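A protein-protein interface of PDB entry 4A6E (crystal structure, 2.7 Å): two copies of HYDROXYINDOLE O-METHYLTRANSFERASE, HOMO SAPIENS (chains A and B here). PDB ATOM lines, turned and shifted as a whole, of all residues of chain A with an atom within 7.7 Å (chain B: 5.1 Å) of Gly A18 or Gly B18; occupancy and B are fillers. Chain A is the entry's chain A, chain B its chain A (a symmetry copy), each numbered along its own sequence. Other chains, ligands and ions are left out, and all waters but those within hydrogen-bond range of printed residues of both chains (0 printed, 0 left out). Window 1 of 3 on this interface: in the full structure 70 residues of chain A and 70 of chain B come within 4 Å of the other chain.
The side-chain hydroxyl of Ser B22 lies within hydrogen-bond range of the backbone carbonyl oxygen of Tyr A15 (2.6 Å).
The side-chain hydroxyl (OG) of Ser B22 is in hydrogen-bond range of the backbone carbonyl oxygen (O) of Ala A16 (3.4 Å).
The backbone NH (N) of Gly A18 sits at hydrogen-bond distance from the side-chain hydroxyl (OG) of Ser B22 (3.2 Å).
The backbone NH of Phe A19 sits at hydrogen-bond distance from the side-chain hydroxyl of Ser B22 (2.9 Å).
The side-chain hydroxyl (OG) of Ser A22 is in hydrogen-bond range of the backbone carbonyl oxygen (O) of Tyr B15.
The side-chain hydroxyl of Ser A22 sits at hydrogen-bond distance from the backbone carbonyl oxygen of Ala B16 (3.4 Å).
OG of Ser A22 is in hydrogen-bond range of N of Gly B18 (3.2 Å).
OG of Ser A22 lies within hydrogen-bond range of N of Phe B19 (2.9 Å).
Tyr A15 touches Val B21, and with the chains exchanged Val A21 touches Tyr B15.
Ala A16 touches Ser B22, and with the chains exchanged Ser A22 touches Ala B16.
Gly B18 touches its own counterpart, Gly A18.
Gly A18 touches Phe B19, and with the chains exchanged Phe A19 touches Gly B18.
10 positions are printed for both chains.
Of the 18 pairs that touch across the chains among the printed residues, 14 have their exchanged pair printed and touching as well.
Val B21 touches Tyr A15.
Gly B18 touches Gly A18 (C to C, 3.6 Å).
N of Phe B19 touches O of Gly A18, at 3.8 Å.
Phe A19 touches Gly B18 (N to O, 3.8 Å).
Phe A19 touches Phe B19.
Tyr B15 touches Val A21 (CD1 to CG1, 3.7 Å).
CZ of Phe A26 touches O of Ala B16 (3.4 Å).
CA of Tyr A114 touches CE2 of Phe B19, at 3.5 Å.
Met B20 touches Leu A298.
Leu A298 touches Val B21.
Gly A18 touches three residues of chain B.
Gly B18 touches three residues of chain A.
Of the printed residues of chain B, Tyr A114 touches Phe B19 (3.5 Å).
Of the printed residues of chain B, Val A21 touches Tyr B15 (3.7 Å).
Printed residues of chain A within 4 Å of Phe B19: Gly A18 (3.8 Å), Phe A19 (3.7 Å), Ser A22 (2.9 Å) and Tyr A114 (3.5 Å).
Asp B14 touches none of the printed residues of chain A.
The nearest residue of chain B that does not touch Gly A18 is Tyr B15 (4.7 Å).
The nearest residue of chain A that does not touch Gly B18 is Tyr A15 (4.7 Å).
The nearest printed residue of chain A that does not touch Ser B22 is Asn A17 (4.1 Å).
The backbone carbonyl oxygen (O) of Gly A18 is in hydrogen-bond range of the side-chain hydroxyl (OG) of Ser A22.
O of Gly B18 sits at hydrogen-bond distance from OG of Ser B22 (3.4 Å).
Of the 16 printed residues of chain A, 9 touch a printed residue of chain B.
Printed residues of chain A that touch a printed residue of chain B: Tyr A15, Ala A16, Gly A18, Phe A19, Val A21, Ser A22, Phe A26, Tyr A114 and Leu A298.
Hydrophobic or aromatic side chains of chain A within 4 Å of the printed part of chain B: Tyr A15, Phe A19, Val A21, Phe A26, Tyr A114 and Leu A298.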
ATOM      1  N   LEU A  12     -11.160  -0.588  -5.532  1.00  0.00           N
ATOM      2  CA  LEU A  12     -10.449  -1.787  -5.953  1.00  0.00           C
ATOM      3  C   LEU A  12     -10.000  -1.693  -7.426  1.00  0.00           C
ATOM      4  O   LEU A  12      -8.845  -2.029  -7.731  1.00  0.00           O
ATOM      5  CB  LEU A  12     -11.326  -3.024  -5.738  1.00  0.00           C
ATOM      6  CG  LEU A  12     -10.631  -4.359  -5.979  1.00  0.00           C
ATOM      7  CD1 LEU A  12      -9.397  -4.529  -5.066  1.00  0.00           C
ATOM      8  CD2 LEU A  12     -11.606  -5.499  -5.882  1.00  0.00           C
ATOM      9  N   ASN A  13     -10.887  -1.201  -8.318  1.00  0.00           N
ATOM     10  CA  ASN A  13     -10.565  -1.031  -9.736  1.00  0.00           C
ATOM     11  C   ASN A  13      -9.526   0.051  -9.953  1.00  0.00           C
ATOM     12  O   ASN A  13      -8.618  -0.126 -10.758  1.00  0.00           O
ATOM     13  CB  ASN A  13     -11.825  -0.807 -10.559  1.00  0.00           C
ATOM     14  CG  ASN A  13     -12.563  -2.109 -10.742  1.00  0.00           C
ATOM     15  OD1 ASN A  13     -12.296  -2.877 -11.676  1.00  0.00           O
ATOM     16  ND2 ASN A  13     -13.414  -2.447  -9.783  1.00  0.00           N
ATOM     17  N   ASP A  14      -9.604   1.131  -9.177  1.00  0.00           N
ATOM     18  CA  ASP A  14      -8.623   2.200  -9.229  1.00  0.00           C
ATOM     19  C   ASP A  14      -7.252   1.601  -9.045  1.00  0.00           C
ATOM     20  O   ASP A  14      -6.382   1.761  -9.911  1.00  0.00           O
ATOM     21  CB  ASP A  14      -8.892   3.243  -8.133  1.00  0.00           C
ATOM     22  CG  ASP A  14     -10.112   4.110  -8.382  1.00  0.00           C
ATOM     23  OD1 ASP A  14     -10.672   4.048  -9.510  1.00  0.00           O
ATOM     24  OD2 ASP A  14     -10.517   4.846  -7.448  1.00  0.00           O
ATOM     25  N   TYR A  15      -7.094   0.836  -7.954  1.00  0.00           N
ATOM     26  CA  TYR A  15      -5.832   0.176  -7.611  1.00  0.00           C
ATOM     27  C   TYR A  15      -5.402  -0.747  -8.715  1.00  0.00           C
ATOM     28  O   TYR A  15      -4.300  -0.590  -9.228  1.00  0.00           O
ATOM     29  CB  TYR A  15      -5.965  -0.587  -6.280  1.00  0.00           C
ATOM     30  CG  TYR A  15      -6.218   0.283  -5.068  1.00  0.00           C
ATOM     31  CD1 TYR A  15      -5.844   1.624  -5.056  1.00  0.00           C
ATOM     32  CD2 TYR A  15      -6.737  -0.258  -3.901  1.00  0.00           C
ATOM     33  CE1 TYR A  15      -6.010   2.412  -3.925  1.00  0.00           C
ATOM     34  CE2 TYR A  15      -6.915   0.523  -2.760  1.00  0.00           C
ATOM     35  CZ  TYR A  15      -6.533   1.858  -2.771  1.00  0.00           C
ATOM     36  OH  TYR A  15      -6.709   2.656  -1.660  1.00  0.00           O
ATOM     37  N   ALA A  16      -6.293  -1.660  -9.132  1.00  0.00           N
ATOM     38  CA  ALA A  16      -6.025  -2.628 -10.192  1.00  0.00           C
ATOM     39  C   ALA A  16      -5.559  -1.992 -11.502  1.00  0.00           C
ATOM     40  O   ALA A  16      -4.711  -2.552 -12.193  1.00  0.00           O
ATOM     41  CB  ALA A  16      -7.269  -3.461 -10.441  1.00  0.00           C
ATOM     42  N   ASN A  17      -6.121  -0.828 -11.841  1.00  0.00           N
ATOM     43  CA  ASN A  17      -5.892  -0.148 -13.111  1.00  0.00           C
ATOM     44  C   ASN A  17      -4.726   0.807 -13.109  1.00  0.00           C
ATOM     45  O   ASN A  17      -4.395   1.352 -14.161  1.00  0.00           O
ATOM     46  CB  ASN A  17      -7.186   0.565 -13.557  1.00  0.00           C
ATOM     47  CG  ASN A  17      -8.384  -0.347 -13.826  1.00  0.00           C
ATOM     48  OD1 ASN A  17      -9.514   0.120 -13.953  1.00  0.00           O
ATOM     49  ND2 ASN A  17      -8.188  -1.662 -13.913  1.00  0.00           N
ATOM     50  N   GLY A  18      -4.131   1.008 -11.933  1.00  0.00           N
ATOM     51  CA  GLY A  18      -2.999   1.896 -11.693  1.00  0.00           C
ATOM     52  C   GLY A  18      -1.829   1.718 -12.641  1.00  0.00           C
ATOM     53  O   GLY A  18      -1.294   2.720 -13.131  1.00  0.00           O
ATOM     54  N   PHE A  19      -1.440   0.455 -12.936  1.00  0.00           N
ATOM     55  CA  PHE A  19      -0.340   0.182 -13.867  1.00  0.00           C
ATOM     56  C   PHE A  19      -0.608   0.673 -15.294  1.00  0.00           C
ATOM     57  O   PHE A  19       0.353   0.955 -16.022  1.00  0.00           O
ATOM     58  CB  PHE A  19       0.031  -1.304 -13.883  1.00  0.00           C
ATOM     59  CG  PHE A  19      -0.916  -2.164 -14.683  1.00  0.00           C
ATOM     60  CD1 PHE A  19      -2.106  -2.617 -14.127  1.00  0.00           C
ATOM     61  CD2 PHE A  19      -0.612  -2.533 -15.990  1.00  0.00           C
ATOM     62  CE1 PHE A  19      -2.972  -3.422 -14.862  1.00  0.00           C
ATOM     63  CE2 PHE A  19      -1.485  -3.331 -16.726  1.00  0.00           C
ATOM     64  CZ  PHE A  19      -2.655  -3.774 -16.155  1.00  0.00           C
ATOM     65  N   MET A  20      -1.906   0.726 -15.707  1.00  0.00           N
ATOM     66  CA  MET A  20      -2.289   1.187 -17.053  1.00  0.00           C
ATOM     67  C   MET A  20      -2.088   2.691 -17.126  1.00  0.00           C
ATOM     68  O   MET A  20      -1.474   3.165 -18.080  1.00  0.00           O
ATOM     69  CB  MET A  20      -3.728   0.786 -17.422  1.00  0.00           C
ATOM     70  CG  MET A  20      -3.918  -0.685 -17.463  1.00  0.00           C
ATOM     71  SD  MET A  20      -5.490  -1.234 -18.147  1.00  0.00           S
ATOM     72  CE  MET A  20      -6.463  -1.292 -16.729  1.00  0.00           C
ATOM     73  N   VAL A  21      -2.528   3.423 -16.071  1.00  0.00           N
ATOM     74  CA  VAL A  21      -2.395   4.878 -15.946  1.00  0.00           C
ATOM     75  C   VAL A  21      -0.911   5.292 -15.921  1.00  0.00           C
ATOM     76  O   VAL A  21      -0.538   6.242 -16.610  1.00  0.00           O
ATOM     77  CB  VAL A  21      -3.211   5.412 -14.739  1.00  0.00           C
ATOM     78  CG1 VAL A  21      -2.866   6.862 -14.411  1.00  0.00           C
ATOM     79  CG2 VAL A  21      -4.699   5.276 -15.003  1.00  0.00           C
ATOM     80  N   SER A  22      -0.067   4.558 -15.160  1.00  0.00           N
ATOM     81  CA  SER A  22       1.377   4.809 -15.076  1.00  0.00           C
ATOM     82  C   SER A  22       2.000   4.724 -16.476  1.00  0.00           C
ATOM     83  O   SER A  22       2.666   5.666 -16.926  1.00  0.00           O
ATOM     84  CB  SER A  22       2.048   3.797 -14.152  1.00  0.00           C
ATOM     85  OG  SER A  22       1.784   4.141 -12.807  1.00  0.00           O
ATOM     86  N   GLN A  23       1.691   3.643 -17.197  1.00  0.00           N
ATOM     87  CA  GLN A  23       2.243   3.454 -18.526  1.00  0.00           C
ATOM     88  C   GLN A  23       1.713   4.405 -19.616  1.00  0.00           C
ATOM     89  O   GLN A  23       2.452   4.704 -20.545  1.00  0.00           O
ATOM     90  CB  GLN A  23       2.321   1.983 -18.914  1.00  0.00           C
ATOM     91  CG  GLN A  23       3.494   1.731 -19.829  1.00  0.00           C
ATOM     92  CD  GLN A  23       4.753   1.397 -19.121  1.00  0.00           C
ATOM     93  OE1 GLN A  23       4.762   0.609 -18.178  1.00  0.00           O
ATOM     94  NE2 GLN A  23       5.860   1.937 -19.613  1.00  0.00           N
ATOM     95  N   VAL A  24       0.502   4.965 -19.454  1.00  0.00           N
ATOM     96  CA  VAL A  24      -0.026   5.979 -20.383  1.00  0.00           C
ATOM     97  C   VAL A  24       0.891   7.223 -20.261  1.00  0.00           C
ATOM     98  O   VAL A  24       1.299   7.779 -21.285  1.00  0.00           O
ATOM     99  CB  VAL A  24      -1.508   6.339 -20.090  1.00  0.00           C
ATOM    100  CG1 VAL A  24      -1.945   7.576 -20.867  1.00  0.00           C
ATOM    101  CG2 VAL A  24      -2.423   5.164 -20.400  1.00  0.00           C
ATOM    102  N   PHE A  26       4.087   7.279 -18.936  1.00  0.00           N
ATOM    103  CA  PHE A  26       5.440   6.899 -19.327  1.00  0.00           C
ATOM    104  C   PHE A  26       5.553   6.882 -20.838  1.00  0.00           C
ATOM    105  O   PHE A  26       6.499   7.454 -21.376  1.00  0.00           O
ATOM    106  CB  PHE A  26       5.840   5.534 -18.735  1.00  0.00           C
ATOM    107  CG  PHE A  26       5.774   5.406 -17.230  1.00  0.00           C
ATOM    108  CD1 PHE A  26       5.904   6.532 -16.404  1.00  0.00           C
ATOM    109  CD2 PHE A  26       5.608   4.162 -16.630  1.00  0.00           C
ATOM    110  CE1 PHE A  26       5.818   6.418 -15.012  1.00  0.00           C
ATOM    111  CE2 PHE A  26       5.560   4.044 -15.234  1.00  0.00           C
ATOM    112  CZ  PHE A  26       5.660   5.178 -14.432  1.00  0.00           C
ATOM    113  N   TYR A 114       9.374  -0.479 -13.377  1.00  0.00           N
ATOM    114  CA  TYR A 114       8.150  -1.175 -13.823  1.00  0.00           C
ATOM    115  C   TYR A 114       8.386  -2.672 -14.058  1.00  0.00           C
ATOM    116  O   TYR A 114       7.588  -3.488 -13.594  1.00  0.00           O
ATOM    117  CB  TYR A 114       7.574  -0.522 -15.096  1.00  0.00           C
ATOM    118  CG  TYR A 114       6.240  -1.093 -15.534  1.00  0.00           C
ATOM    119  CD1 TYR A 114       6.175  -2.222 -16.361  1.00  0.00           C
ATOM    120  CD2 TYR A 114       5.042  -0.499 -15.143  1.00  0.00           C
ATOM    121  CE1 TYR A 114       4.950  -2.738 -16.789  1.00  0.00           C
ATOM    122  CE2 TYR A 114       3.810  -1.009 -15.564  1.00  0.00           C
ATOM    123  CZ  TYR A 114       3.770  -2.144 -16.366  1.00  0.00           C
ATOM    124  OH  TYR A 114       2.569  -2.642 -16.790  1.00  0.00           O
ATOM    125  N   LEU A 298       6.020   2.967  -0.613  1.00  0.00           N
ATOM    126  CA  LEU A 298       6.219   2.412  -1.943  1.00  0.00           C
ATOM    127  C   LEU A 298       7.674   2.480  -2.328  1.00  0.00           C
ATOM    128  O   LEU A 298       8.205   1.483  -2.830  1.00  0.00           O
ATOM    129  CB  LEU A 298       5.299   3.075  -2.989  1.00  0.00           C
ATOM    130  CG  LEU A 298       3.792   2.886  -2.754  1.00  0.00           C
ATOM    131  CD1 LEU A 298       3.005   3.822  -3.569  1.00  0.00           C
ATOM    132  CD2 LEU A 298       3.349   1.464  -3.021  1.00  0.00           C
ATOM    133  N   ASN B  13       2.815  12.382  -9.223  1.00  0.00           N
ATOM    134  CA  ASN B  13       3.394  11.257  -8.485  1.00  0.00           C
ATOM    135  C   ASN B  13       2.398  10.131  -8.300  1.00  0.00           C
ATOM    136  O   ASN B  13       2.755   8.967  -8.451  1.00  0.00           O
ATOM    137  CB  ASN B  13       4.003  11.723  -7.171  1.00  0.00           C
ATOM    138  CG  ASN B  13       5.321  12.412  -7.425  1.00  0.00           C
ATOM    139  OD1 ASN B  13       6.380  11.775  -7.493  1.00  0.00           O
ATOM    140  ND2 ASN B  13       5.267  13.708  -7.701  1.00  0.00           N
ATOM    141  N   ASP B  14       1.132  10.473  -8.062  1.00  0.00           N
ATOM    142  CA  ASP B  14       0.068   9.492  -7.947  1.00  0.00           C
ATOM    143  C   ASP B  14       0.084   8.622  -9.178  1.00  0.00           C
ATOM    144  O   ASP B  14       0.220   7.396  -9.072  1.00  0.00           O
ATOM    145  CB  ASP B  14      -1.298  10.181  -7.807  1.00  0.00           C
ATOM    146  CG  ASP B  14      -1.528  10.849  -6.464  1.00  0.00           C
ATOM    147  OD1 ASP B  14      -0.701  10.630  -5.537  1.00  0.00           O
ATOM    148  OD2 ASP B  14      -2.526  11.599  -6.338  1.00  0.00           O
ATOM    149  N   TYR B  15       0.032   9.274 -10.350  1.00  0.00           N
ATOM    150  CA  TYR B  15       0.035   8.595 -11.648  1.00  0.00           C
ATOM    151  C   TYR B  15       1.270   7.755 -11.801  1.00  0.00           C
ATOM    152  O   TYR B  15       1.151   6.556 -12.031  1.00  0.00           O
ATOM    153  CB  TYR B  15      -0.077   9.618 -12.793  1.00  0.00           C
ATOM    154  CG  TYR B  15      -1.376  10.392 -12.833  1.00  0.00           C
ATOM    155  CD1 TYR B  15      -2.535   9.881 -12.252  1.00  0.00           C
ATOM    156  CD2 TYR B  15      -1.473  11.584 -13.536  1.00  0.00           C
ATOM    157  CE1 TYR B  15      -3.746  10.553 -12.343  1.00  0.00           C
ATOM    158  CE2 TYR B  15      -2.681  12.272 -13.629  1.00  0.00           C
ATOM    159  CZ  TYR B  15      -3.823  11.742 -13.045  1.00  0.00           C
ATOM    160  OH  TYR B  15      -5.029  12.408 -13.111  1.00  0.00           O
ATOM    161  N   ALA B  16       2.452   8.360 -11.604  1.00  0.00           N
ATOM    162  CA  ALA B  16       3.739   7.680 -11.719  1.00  0.00           C
ATOM    163  C   ALA B  16       3.854   6.430 -10.847  1.00  0.00           C
ATOM    164  O   ALA B  16       4.465   5.445 -11.258  1.00  0.00           O
ATOM    165  CB  ALA B  16       4.854   8.650 -11.372  1.00  0.00           C
ATOM    166  N   ASN B  17       3.273   6.476  -9.645  1.00  0.00           N
ATOM    167  CA  ASN B  17       3.392   5.427  -8.637  1.00  0.00           C
ATOM    168  C   ASN B  17       2.340   4.352  -8.725  1.00  0.00           C
ATOM    169  O   ASN B  17       2.415   3.376  -7.981  1.00  0.00           O
ATOM    170  CB  ASN B  17       3.413   6.062  -7.231  1.00  0.00           C
ATOM    171  CG  ASN B  17       4.590   6.997  -6.945  1.00  0.00           C
ATOM    172  OD1 ASN B  17       4.585   7.733  -5.961  1.00  0.00           O
ATOM    173  ND2 ASN B  17       5.623   7.011  -7.786  1.00  0.00           N
ATOM    174  N   GLY B  18       1.368   4.550  -9.617  1.00  0.00           N
ATOM    175  CA  GLY B  18       0.245   3.654  -9.863  1.00  0.00           C
ATOM    176  C   GLY B  18       0.616   2.200 -10.079  1.00  0.00           C
ATOM    177  O   GLY B  18      -0.035   1.320  -9.502  1.00  0.00           O
ATOM    178  N   PHE B  19       1.674   1.928 -10.878  1.00  0.00           N
ATOM    179  CA  PHE B  19       2.130   0.555 -11.121  1.00  0.00           C
ATOM    180  C   PHE B  19       2.612  -0.164  -9.857  1.00  0.00           C
ATOM    181  O   PHE B  19       2.552  -1.400  -9.809  1.00  0.00           O
ATOM    182  CB  PHE B  19       3.211   0.501 -12.203  1.00  0.00           C
ATOM    183  CG  PHE B  19       4.580   0.914 -11.722  1.00  0.00           C
ATOM    184  CD1 PHE B  19       4.932   2.256 -11.644  1.00  0.00           C
ATOM    185  CD2 PHE B  19       5.526  -0.039 -11.358  1.00  0.00           C
ATOM    186  CE1 PHE B  19       6.200   2.635 -11.212  1.00  0.00           C
ATOM    187  CE2 PHE B  19       6.792   0.343 -10.919  1.00  0.00           C
ATOM    188  CZ  PHE B  19       7.121   1.677 -10.854  1.00  0.00           C
ATOM    189  N   MET B  20       3.136   0.603  -8.859  1.00  0.00           N
ATOM    190  CA  MET B  20       3.627   0.028  -7.595  1.00  0.00           C
ATOM    191  C   MET B  20       2.434  -0.424  -6.771  1.00  0.00           C
ATOM    192  O   MET B  20       2.438  -1.553  -6.285  1.00  0.00           O
ATOM    193  CB  MET B  20       4.520   1.008  -6.813  1.00  0.00           C
ATOM    194  CG  MET B  20       5.749   1.378  -7.556  1.00  0.00           C
ATOM    195  SD  MET B  20       6.969   2.300  -6.606  1.00  0.00           S
ATOM    196  CE  MET B  20       6.468   3.918  -6.912  1.00  0.00           C
ATOM    197  N   VAL B  21       1.378   0.427  -6.697  1.00  0.00           N
ATOM    198  CA  VAL B  21       0.129   0.154  -5.980  1.00  0.00           C
ATOM    199  C   VAL B  21      -0.592  -1.068  -6.581  1.00  0.00           C
ATOM    200  O   VAL B  21      -1.049  -1.929  -5.829  1.00  0.00           O
ATOM    201  CB  VAL B  21      -0.759   1.424  -5.900  1.00  0.00           C
ATOM    202  CG1 VAL B  21      -2.172   1.106  -5.420  1.00  0.00           C
ATOM    203  CG2 VAL B  21      -0.121   2.461  -4.993  1.00  0.00           C
ATOM    204  N   SER B  22      -0.659  -1.157  -7.929  1.00  0.00           N
ATOM    205  CA  SER B  22      -1.275  -2.286  -8.639  1.00  0.00           C
ATOM    206  C   SER B  22      -0.582  -3.594  -8.232  1.00  0.00           C
ATOM    207  O   SER B  22      -1.242  -4.542  -7.786  1.00  0.00           O
ATOM    208  CB  SER B  22      -1.169  -2.096 -10.149  1.00  0.00           C
ATOM    209  OG  SER B  22      -2.126  -1.146 -10.571  1.00  0.00           O
